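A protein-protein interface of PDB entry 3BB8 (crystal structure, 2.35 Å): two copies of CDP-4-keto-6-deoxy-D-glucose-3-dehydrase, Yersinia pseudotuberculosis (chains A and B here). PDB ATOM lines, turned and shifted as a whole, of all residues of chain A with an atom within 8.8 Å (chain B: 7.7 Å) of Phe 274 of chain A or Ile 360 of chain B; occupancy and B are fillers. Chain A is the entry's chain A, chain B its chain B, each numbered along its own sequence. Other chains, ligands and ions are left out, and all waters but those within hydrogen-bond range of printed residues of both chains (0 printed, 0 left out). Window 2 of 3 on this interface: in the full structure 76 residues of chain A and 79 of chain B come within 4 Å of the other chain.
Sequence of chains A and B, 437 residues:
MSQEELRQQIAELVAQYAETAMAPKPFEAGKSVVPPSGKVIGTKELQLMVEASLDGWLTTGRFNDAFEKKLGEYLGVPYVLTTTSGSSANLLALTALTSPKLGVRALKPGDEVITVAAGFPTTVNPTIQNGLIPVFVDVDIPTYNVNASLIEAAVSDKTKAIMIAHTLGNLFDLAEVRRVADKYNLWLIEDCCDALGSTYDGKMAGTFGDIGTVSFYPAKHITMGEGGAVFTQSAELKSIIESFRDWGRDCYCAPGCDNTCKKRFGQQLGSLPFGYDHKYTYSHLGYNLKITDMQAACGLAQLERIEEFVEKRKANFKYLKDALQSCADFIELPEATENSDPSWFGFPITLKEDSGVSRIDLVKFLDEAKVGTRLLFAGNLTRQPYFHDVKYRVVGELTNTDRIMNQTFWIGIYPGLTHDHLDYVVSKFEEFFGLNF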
ATOM      1  N   GLN A 268      -6.954   6.628  25.571  1.00  0.00           N
ATOM      2  CA  GLN A 268      -7.480   6.935  24.244  1.00  0.00           C
ATOM      3  C   GLN A 268      -6.447   7.600  23.332  1.00  0.00           C
ATOM      4  O   GLN A 268      -5.432   8.126  23.796  1.00  0.00           O
ATOM      5  CB  GLN A 268      -8.727   7.823  24.361  1.00  0.00           C
ATOM      6  CG  GLN A 268      -8.963   8.424  25.747  1.00  0.00           C
ATOM      7  CD  GLN A 268      -7.943   9.488  26.122  1.00  0.00           C
ATOM      8  OE1 GLN A 268      -8.027  10.092  27.194  1.00  0.00           O
ATOM      9  NE2 GLN A 268      -6.976   9.725  25.239  1.00  0.00           N
ATOM     10  N   SER A 271      -4.726  13.791  20.726  1.00  0.00           N
ATOM     11  CA  SER A 271      -4.322  14.709  21.777  1.00  0.00           C
ATOM     12  C   SER A 271      -5.329  15.844  21.912  1.00  0.00           C
ATOM     13  O   SER A 271      -4.960  17.018  21.947  1.00  0.00           O
ATOM     14  CB  SER A 271      -2.940  15.274  21.465  1.00  0.00           C
ATOM     15  OG  SER A 271      -2.930  15.882  20.193  1.00  0.00           O
ATOM     16  N   LEU A 272      -6.606  15.484  21.977  1.00  0.00           N
ATOM     17  CA  LEU A 272      -7.666  16.469  22.120  1.00  0.00           C
ATOM     18  C   LEU A 272      -7.748  16.915  23.572  1.00  0.00           C
ATOM     19  O   LEU A 272      -7.481  16.132  24.488  1.00  0.00           O
ATOM     20  CB  LEU A 272      -9.019  15.877  21.701  1.00  0.00           C
ATOM     21  CG  LEU A 272      -9.266  15.578  20.221  1.00  0.00           C
ATOM     22  CD1 LEU A 272     -10.641  14.937  20.057  1.00  0.00           C
ATOM     23  CD2 LEU A 272      -9.162  16.865  19.405  1.00  0.00           C
ATOM     24  N   PRO A 273      -8.126  18.181  23.804  1.00  0.00           N
ATOM     25  CA  PRO A 273      -8.235  18.688  25.173  1.00  0.00           C
ATOM     26  C   PRO A 273      -9.349  17.976  25.932  1.00  0.00           C
ATOM     27  O   PRO A 273     -10.314  17.500  25.336  1.00  0.00           O
ATOM     28  CB  PRO A 273      -8.527  20.175  24.965  1.00  0.00           C
ATOM     29  CG  PRO A 273      -9.299  20.181  23.682  1.00  0.00           C
ATOM     30  CD  PRO A 273      -8.506  19.217  22.829  1.00  0.00           C
ATOM     31  N   PHE A 274      -9.203  17.896  27.248  1.00  0.00           N
ATOM     32  CA  PHE A 274     -10.205  17.259  28.086  1.00  0.00           C
ATOM     33  C   PHE A 274     -11.556  17.946  27.900  1.00  0.00           C
ATOM     34  O   PHE A 274     -11.627  19.172  27.774  1.00  0.00           O
ATOM     35  CB  PHE A 274      -9.767  17.329  29.555  1.00  0.00           C
ATOM     36  CG  PHE A 274     -10.853  16.984  30.533  1.00  0.00           C
ATOM     37  CD1 PHE A 274     -11.737  17.959  30.984  1.00  0.00           C
ATOM     38  CD2 PHE A 274     -11.013  15.677  30.980  1.00  0.00           C
ATOM     39  CE1 PHE A 274     -12.767  17.636  31.864  1.00  0.00           C
ATOM     40  CE2 PHE A 274     -12.040  15.343  31.859  1.00  0.00           C
ATOM     41  CZ  PHE A 274     -12.920  16.325  32.301  1.00  0.00           C
ATOM     42  N   GLY A 275     -12.625  17.156  27.868  1.00  0.00           N
ATOM     43  CA  GLY A 275     -13.954  17.718  27.710  1.00  0.00           C
ATOM     44  C   GLY A 275     -14.368  18.073  26.289  1.00  0.00           C
ATOM     45  O   GLY A 275     -15.437  18.661  26.088  1.00  0.00           O
ATOM     46  N   TYR A 276     -13.538  17.736  25.304  1.00  0.00           N
ATOM     47  CA  TYR A 276     -13.877  18.031  23.913  1.00  0.00           C
ATOM     48  C   TYR A 276     -15.130  17.235  23.559  1.00  0.00           C
ATOM     49  O   TYR A 276     -15.225  16.052  23.864  1.00  0.00           O
ATOM     50  CB  TYR A 276     -12.735  17.633  22.969  1.00  0.00           C
ATOM     51  CG  TYR A 276     -12.744  18.399  21.671  1.00  0.00           C
ATOM     52  CD1 TYR A 276     -12.176  19.668  21.591  1.00  0.00           C
ATOM     53  CD2 TYR A 276     -13.370  17.878  20.526  1.00  0.00           C
ATOM     54  CE1 TYR A 276     -12.226  20.412  20.413  1.00  0.00           C
ATOM     55  CE2 TYR A 276     -13.428  18.617  19.337  1.00  0.00           C
ATOM     56  CZ  TYR A 276     -12.852  19.884  19.291  1.00  0.00           C
ATOM     57  OH  TYR A 276     -12.899  20.626  18.132  1.00  0.00           O
ATOM     58  N   ASP A 277     -16.085  17.897  22.917  1.00  0.00           N
ATOM     59  CA  ASP A 277     -17.351  17.283  22.525  1.00  0.00           C
ATOM     60  C   ASP A 277     -17.175  15.910  21.868  1.00  0.00           C
ATOM     61  O   ASP A 277     -16.435  15.776  20.893  1.00  0.00           O
ATOM     62  CB  ASP A 277     -18.087  18.222  21.561  1.00  0.00           C
ATOM     63  CG  ASP A 277     -19.584  18.228  21.781  1.00  0.00           C
ATOM     64  OD1 ASP A 277     -20.236  17.190  21.533  1.00  0.00           O
ATOM     65  OD2 ASP A 277     -20.108  19.279  22.211  1.00  0.00           O
ATOM     66  N   LEU B 351     -12.586  32.229  23.710  1.00  0.00           N
ATOM     67  CA  LEU B 351     -12.474  32.703  25.085  1.00  0.00           C
ATOM     68  C   LEU B 351     -11.014  32.891  25.485  1.00  0.00           C
ATOM     69  O   LEU B 351     -10.196  31.986  25.328  1.00  0.00           O
ATOM     70  CB  LEU B 351     -13.161  31.729  26.044  1.00  0.00           C
ATOM     71  CG  LEU B 351     -12.935  31.976  27.538  1.00  0.00           C
ATOM     72  CD1 LEU B 351     -13.867  33.064  28.049  1.00  0.00           C
ATOM     73  CD2 LEU B 351     -13.120  30.690  28.329  1.00  0.00           C
ATOM     74  N   VAL B 357     -11.245  31.493  33.522  1.00  0.00           N
ATOM     75  CA  VAL B 357     -12.133  30.335  33.441  1.00  0.00           C
ATOM     76  C   VAL B 357     -11.826  29.523  32.189  1.00  0.00           C
ATOM     77  O   VAL B 357     -11.128  29.988  31.293  1.00  0.00           O
ATOM     78  CB  VAL B 357     -13.623  30.741  33.423  1.00  0.00           C
ATOM     79  CG1 VAL B 357     -13.980  31.433  34.724  1.00  0.00           C
ATOM     80  CG2 VAL B 357     -13.909  31.636  32.228  1.00  0.00           C
ATOM     81  N   SER B 358     -12.347  28.304  32.138  1.00  0.00           N
ATOM     82  CA  SER B 358     -12.118  27.410  31.006  1.00  0.00           C
ATOM     83  C   SER B 358     -13.345  27.344  30.107  1.00  0.00           C
ATOM     84  O   SER B 358     -14.463  27.587  30.563  1.00  0.00           O
ATOM     85  CB  SER B 358     -11.809  26.007  31.520  1.00  0.00           C
ATOM     86  OG  SER B 358     -12.933  25.497  32.221  1.00  0.00           O
ATOM     87  N   ARG B 359     -13.139  26.993  28.839  1.00  0.00           N
ATOM     88  CA  ARG B 359     -14.251  26.891  27.896  1.00  0.00           C
ATOM     89  C   ARG B 359     -15.333  25.987  28.472  1.00  0.00           C
ATOM     90  O   ARG B 359     -16.519  26.268  28.328  1.00  0.00           O
ATOM     91  CB  ARG B 359     -13.770  26.351  26.541  1.00  0.00           C
ATOM     92  CG  ARG B 359     -14.869  26.245  25.475  1.00  0.00           C
ATOM     93  CD  ARG B 359     -14.302  25.771  24.132  1.00  0.00           C
ATOM     94  NE  ARG B 359     -13.652  24.465  24.251  1.00  0.00           N
ATOM     95  CZ  ARG B 359     -12.799  23.963  23.364  1.00  0.00           C
ATOM     96  NH1 ARG B 359     -12.485  24.649  22.271  1.00  0.00           N
ATOM     97  NH2 ARG B 359     -12.230  22.784  23.591  1.00  0.00           N
ATOM     98  N   ILE B 360     -14.917  24.910  29.131  1.00  0.00           N
ATOM     99  CA  ILE B 360     -15.852  23.971  29.747  1.00  0.00           C
ATOM    100  C   ILE B 360     -16.825  24.702  30.672  1.00  0.00           C
ATOM    101  O   ILE B 360     -18.036  24.456  30.636  1.00  0.00           O
ATOM    102  CB  ILE B 360     -15.109  22.891  30.591  1.00  0.00           C
ATOM    103  CG1 ILE B 360     -14.184  22.061  29.702  1.00  0.00           C
ATOM    104  CG2 ILE B 360     -16.119  21.975  31.270  1.00  0.00           C
ATOM    105  CD1 ILE B 360     -13.536  20.886  30.426  1.00  0.00           C
ATOM    106  N   ASP B 361     -16.292  25.594  31.507  1.00  0.00           N
ATOM    107  CA  ASP B 361     -17.118  26.356  32.442  1.00  0.00           C
ATOM    108  C   ASP B 361     -18.202  27.141  31.722  1.00  0.00           C
ATOM    109  O   ASP B 361     -19.382  27.071  32.081  1.00  0.00           O
ATOM    110  CB  ASP B 361     -16.264  27.344  33.255  1.00  0.00           C
ATOM    111  CG  ASP B 361     -15.217  26.654  34.106  1.00  0.00           C
ATOM    112  OD1 ASP B 361     -15.550  25.618  34.722  1.00  0.00           O
ATOM    113  OD2 ASP B 361     -14.068  27.155  34.165  1.00  0.00           O
ATOM    114  N   LEU B 362     -17.792  27.899  30.711  1.00  0.00           N
ATOM    115  CA  LEU B 362     -18.720  28.713  29.941  1.00  0.00           C
ATOM    116  C   LEU B 362     -19.754  27.847  29.213  1.00  0.00           C
ATOM    117  O   LEU B 362     -20.960  28.112  29.286  1.00  0.00           O
ATOM    118  CB  LEU B 362     -17.938  29.588  28.948  1.00  0.00           C
ATOM    119  CG  LEU B 362     -18.737  30.593  28.106  1.00  0.00           C
ATOM    120  CD1 LEU B 362     -19.640  31.415  29.001  1.00  0.00           C
ATOM    121  CD2 LEU B 362     -17.776  31.503  27.335  1.00  0.00           C
ATOM    122  N   VAL B 363     -19.289  26.807  28.524  1.00  0.00           N
ATOM    123  CA  VAL B 363     -20.207  25.929  27.807  1.00  0.00           C
ATOM    124  C   VAL B 363     -21.223  25.336  28.776  1.00  0.00           C
ATOM    125  O   VAL B 363     -22.424  25.355  28.516  1.00  0.00           O
ATOM    126  CB  VAL B 363     -19.464  24.780  27.101  1.00  0.00           C
ATOM    127  CG1 VAL B 363     -20.471  23.784  26.546  1.00  0.00           C
ATOM    128  CG2 VAL B 363     -18.591  25.332  25.981  1.00  0.00           C
ATOM    129  N   LYS B 364     -20.737  24.820  29.901  1.00  0.00           N
ATOM    130  CA  LYS B 364     -21.628  24.226  30.886  1.00  0.00           C
ATOM    131  C   LYS B 364     -22.594  25.263  31.446  1.00  0.00           C
ATOM    132  O   LYS B 364     -23.749  24.947  31.717  1.00  0.00           O
ATOM    133  CB  LYS B 364     -20.833  23.583  32.025  1.00  0.00           C
ATOM    134  CG  LYS B 364     -21.708  22.815  33.015  1.00  0.00           C
ATOM    135  CD  LYS B 364     -20.872  22.157  34.108  1.00  0.00           C
ATOM    136  CE  LYS B 364     -19.929  21.086  33.547  1.00  0.00           C
ATOM    137  NZ  LYS B 364     -20.660  19.899  33.007  1.00  0.00           N
ATOM    138  N   PHE B 365     -22.124  26.497  31.621  1.00  0.00           N
ATOM    139  CA  PHE B 365     -22.989  27.561  32.130  1.00  0.00           C
ATOM    140  C   PHE B 365     -24.092  27.809  31.107  1.00  0.00           C
ATOM    141  O   PHE B 365     -25.276  27.787  31.438  1.00  0.00           O
ATOM    142  CB  PHE B 365     -22.200  28.859  32.358  1.00  0.00           C
ATOM    143  CG  PHE B 365     -23.063  30.029  32.759  1.00  0.00           C
ATOM    144  CD1 PHE B 365     -23.668  30.072  34.014  1.00  0.00           C
ATOM    145  CD2 PHE B 365     -23.296  31.074  31.872  1.00  0.00           C
ATOM    146  CE1 PHE B 365     -24.494  31.140  34.378  1.00  0.00           C
ATOM    147  CE2 PHE B 365     -24.120  32.149  32.226  1.00  0.00           C
ATOM    148  CZ  PHE B 365     -24.720  32.179  33.482  1.00  0.00           C
ATOM    149  N   LEU B 366     -23.691  28.040  29.862  1.00  0.00           N
ATOM    150  CA  LEU B 366     -24.638  28.287  28.776  1.00  0.00           C
ATOM    151  C   LEU B 366     -25.605  27.128  28.582  1.00  0.00           C
ATOM    152  O   LEU B 366     -26.798  27.329  28.349  1.00  0.00           O
ATOM    153  CB  LEU B 366     -23.877  28.549  27.480  1.00  0.00           C
ATOM    154  CG  LEU B 366     -23.137  29.884  27.498  1.00  0.00           C
ATOM    155  CD1 LEU B 366     -22.278  30.054  26.259  1.00  0.00           C
ATOM    156  CD2 LEU B 366     -24.171  30.984  27.593  1.00  0.00           C
ATOM    157  N   ASP B 367     -25.088  25.913  28.692  1.00  0.00           N
ATOM    158  CA  ASP B 367     -25.904  24.721  28.530  1.00  0.00           C
ATOM    159  C   ASP B 367     -27.056  24.741  29.531  1.00  0.00           C
ATOM    160  O   ASP B 367     -28.200  24.443  29.187  1.00  0.00           O
ATOM    161  CB  ASP B 367     -25.046  23.472  28.749  1.00  0.00           C
ATOM    162  CG  ASP B 367     -25.760  22.192  28.348  1.00  0.00           C
ATOM    163  OD1 ASP B 367     -25.222  21.097  28.634  1.00  0.00           O
ATOM    164  OD2 ASP B 367     -26.851  22.275  27.742  1.00  0.00           O
ATOM    165  N   LEU B 375     -18.306  23.241  19.472  1.00  0.00           N
ATOM    166  CA  LEU B 375     -16.895  23.516  19.283  1.00  0.00           C
ATOM    167  C   LEU B 375     -16.700  23.658  17.771  1.00  0.00           C
ATOM    168  O   LEU B 375     -17.594  23.313  17.002  1.00  0.00           O
ATOM    169  CB  LEU B 375     -16.058  22.362  19.844  1.00  0.00           C
ATOM    170  CG  LEU B 375     -16.224  22.145  21.355  1.00  0.00           C
ATOM    171  CD1 LEU B 375     -15.192  21.133  21.859  1.00  0.00           C
ATOM    172  CD2 LEU B 375     -16.043  23.473  22.078  1.00  0.00           C
ATOM    173  N   MET B 405      -8.971  24.652  18.942  1.00  0.00           N
ATOM    174  CA  MET B 405      -9.355  23.405  19.594  1.00  0.00           C
ATOM    175  C   MET B 405      -9.518  23.597  21.098  1.00  0.00           C
ATOM    176  O   MET B 405     -10.329  22.924  21.735  1.00  0.00           O
ATOM    177  CB  MET B 405      -8.321  22.313  19.313  1.00  0.00           C
ATOM    178  CG  MET B 405      -8.552  21.026  20.086  1.00  0.00           C
ATOM    179  SD  MET B 405      -7.134  19.913  20.027  1.00  0.00           S
ATOM    180  CE  MET B 405      -5.910  20.879  20.909  1.00  0.00           C
ATOM    181  N   ASN B 406      -8.774  24.553  21.656  1.00  0.00           N
ATOM    182  CA  ASN B 406      -8.704  24.710  23.104  1.00  0.00           C
ATOM    183  C   ASN B 406      -9.628  25.815  23.607  1.00  0.00           C
ATOM    184  O   ASN B 406     -10.004  25.777  24.820  1.00  0.00           O
ATOM    185  CB  ASN B 406      -7.267  24.986  23.545  1.00  0.00           C
ATOM    186  CG  ASN B 406      -6.369  23.772  23.398  1.00  0.00           C
ATOM    187  OD1 ASN B 406      -6.840  22.636  23.381  1.00  0.00           O
ATOM    188  ND2 ASN B 406      -5.067  24.010  23.290  1.00  0.00           N
ATOM    189  N   GLN B 407      -9.948  26.772  22.803  1.00  0.00           N
ATOM    190  CA  GLN B 407     -10.605  27.922  23.411  1.00  0.00           C
ATOM    191  C   GLN B 407     -11.825  28.421  22.643  1.00  0.00           C
ATOM    192  O   GLN B 407     -12.522  29.332  23.090  1.00  0.00           O
ATOM    193  CB  GLN B 407      -9.517  28.998  23.424  1.00  0.00           C
ATOM    194  CG  GLN B 407      -8.342  28.680  24.335  1.00  0.00           C
ATOM    195  CD  GLN B 407      -8.733  28.645  25.800  1.00  0.00           C
ATOM    196  OE1 GLN B 407      -9.228  29.631  26.346  1.00  0.00           O
ATOM    197  NE2 GLN B 407      -8.510  27.506  26.445  1.00  0.00           N
ATOM    198  N   PHE B 432     -22.642  35.906  33.189  1.00  0.00           N
ATOM    199  CA  PHE B 432     -21.501  35.022  33.393  1.00  0.00           C
ATOM    200  C   PHE B 432     -20.240  35.785  33.783  1.00  0.00           C
ATOM    201  O   PHE B 432     -19.574  35.440  34.757  1.00  0.00           O
ATOM    202  CB  PHE B 432     -21.212  34.218  32.119  1.00  0.00           C
ATOM    203  CG  PHE B 432     -20.073  33.242  32.258  1.00  0.00           C
ATOM    204  CD1 PHE B 432     -20.264  32.014  32.883  1.00  0.00           C
ATOM    205  CD2 PHE B 432     -18.803  33.556  31.768  1.00  0.00           C
ATOM    206  CE1 PHE B 432     -19.212  31.109  33.015  1.00  0.00           C
ATOM    207  CE2 PHE B 432     -17.744  32.659  31.896  1.00  0.00           C
ATOM    208  CZ  PHE B 432     -17.949  31.433  32.519  1.00  0.00           C
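NH2 of Arg 359 of chain B lies within hydrogen-bond range of O of Met 405 of chain B (2.7 Å).
Leu 272 of chain A touches Met 405 of chain B.
CG of Pro 273 of chain A touches NH2 of Arg 359 of chain B, at 3.9 Å.
SD of Met 405 of chain B touches CD of Pro 273 of chain A, at 3.2 Å.
Pro 273 of chain A touches Asn 406 of chain B.
CD1 of Phe 274 of chain A touches CD1 of Ile 360 of chain B, 3.5 Å away.
NH2 of Arg 359 of chain B touches CD1 of Tyr 276 of chain A (3.7 Å).
CD1 of Tyr 276 of chain A touches CD1 of Leu 375 of chain B, 3.4 Å away.
O of Met 405 of chain B touches CE1 of Tyr 276 of chain A, 3.4 Å away.
N of Asp 277 of chain A touches CD1 of Leu 375 of chain B (3.5 Å).
Printed residues of chain B within 4 Å of Leu 272 of chain A: Met 405.
Phe 274 of chain A touches one residue of chain B.
Of the printed residues of chain B, Tyr 276 of chain A touches Arg 359 (3.7 Å), Leu 375 (3.4 Å) and Met 405 (3.4 Å).
Of the printed residues of chain B, Asp 277 of chain A touches Leu 375.
Ile 360 of chain B touches one residue of chain A.
Printed residues of chain A within 4 Å of Leu 375 of chain B: Tyr 276 and Asp 277.
Of the printed residues of chain A, Met 405 of chain B touches Leu 272 (3.7 Å), Pro 273 (3.2 Å) and Tyr 276 (3.4 Å).
The nearest residue of chain B that does not touch Phe 274 of chain A is Arg 359 of chain B (5.6 Å).
The nearest printed residue of chain B that does not touch Tyr 276 of chain A is Asn 406 of chain B (5.5 Å).
Of the 8 printed residues of chain A, 5 touch a printed residue of chain B.
Hydrophobic or aromatic side chains of chain A within 4 Å of the printed part of chain B: Leu 272, Pro 273, Phe 274 and Tyr 276.
Of the 17 printed residues of chain B, 5 touch a printed residue of chain A.
Printed residues of chain B that touch a printed residue of chain A: Arg 359, Ile 360, Leu 375, Met 405 and Asn 406.
No position is printed for both chains.
Of the 9 pairs that touch across the chains among the printed residues, none has its exchanged pair printed and touching as well.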
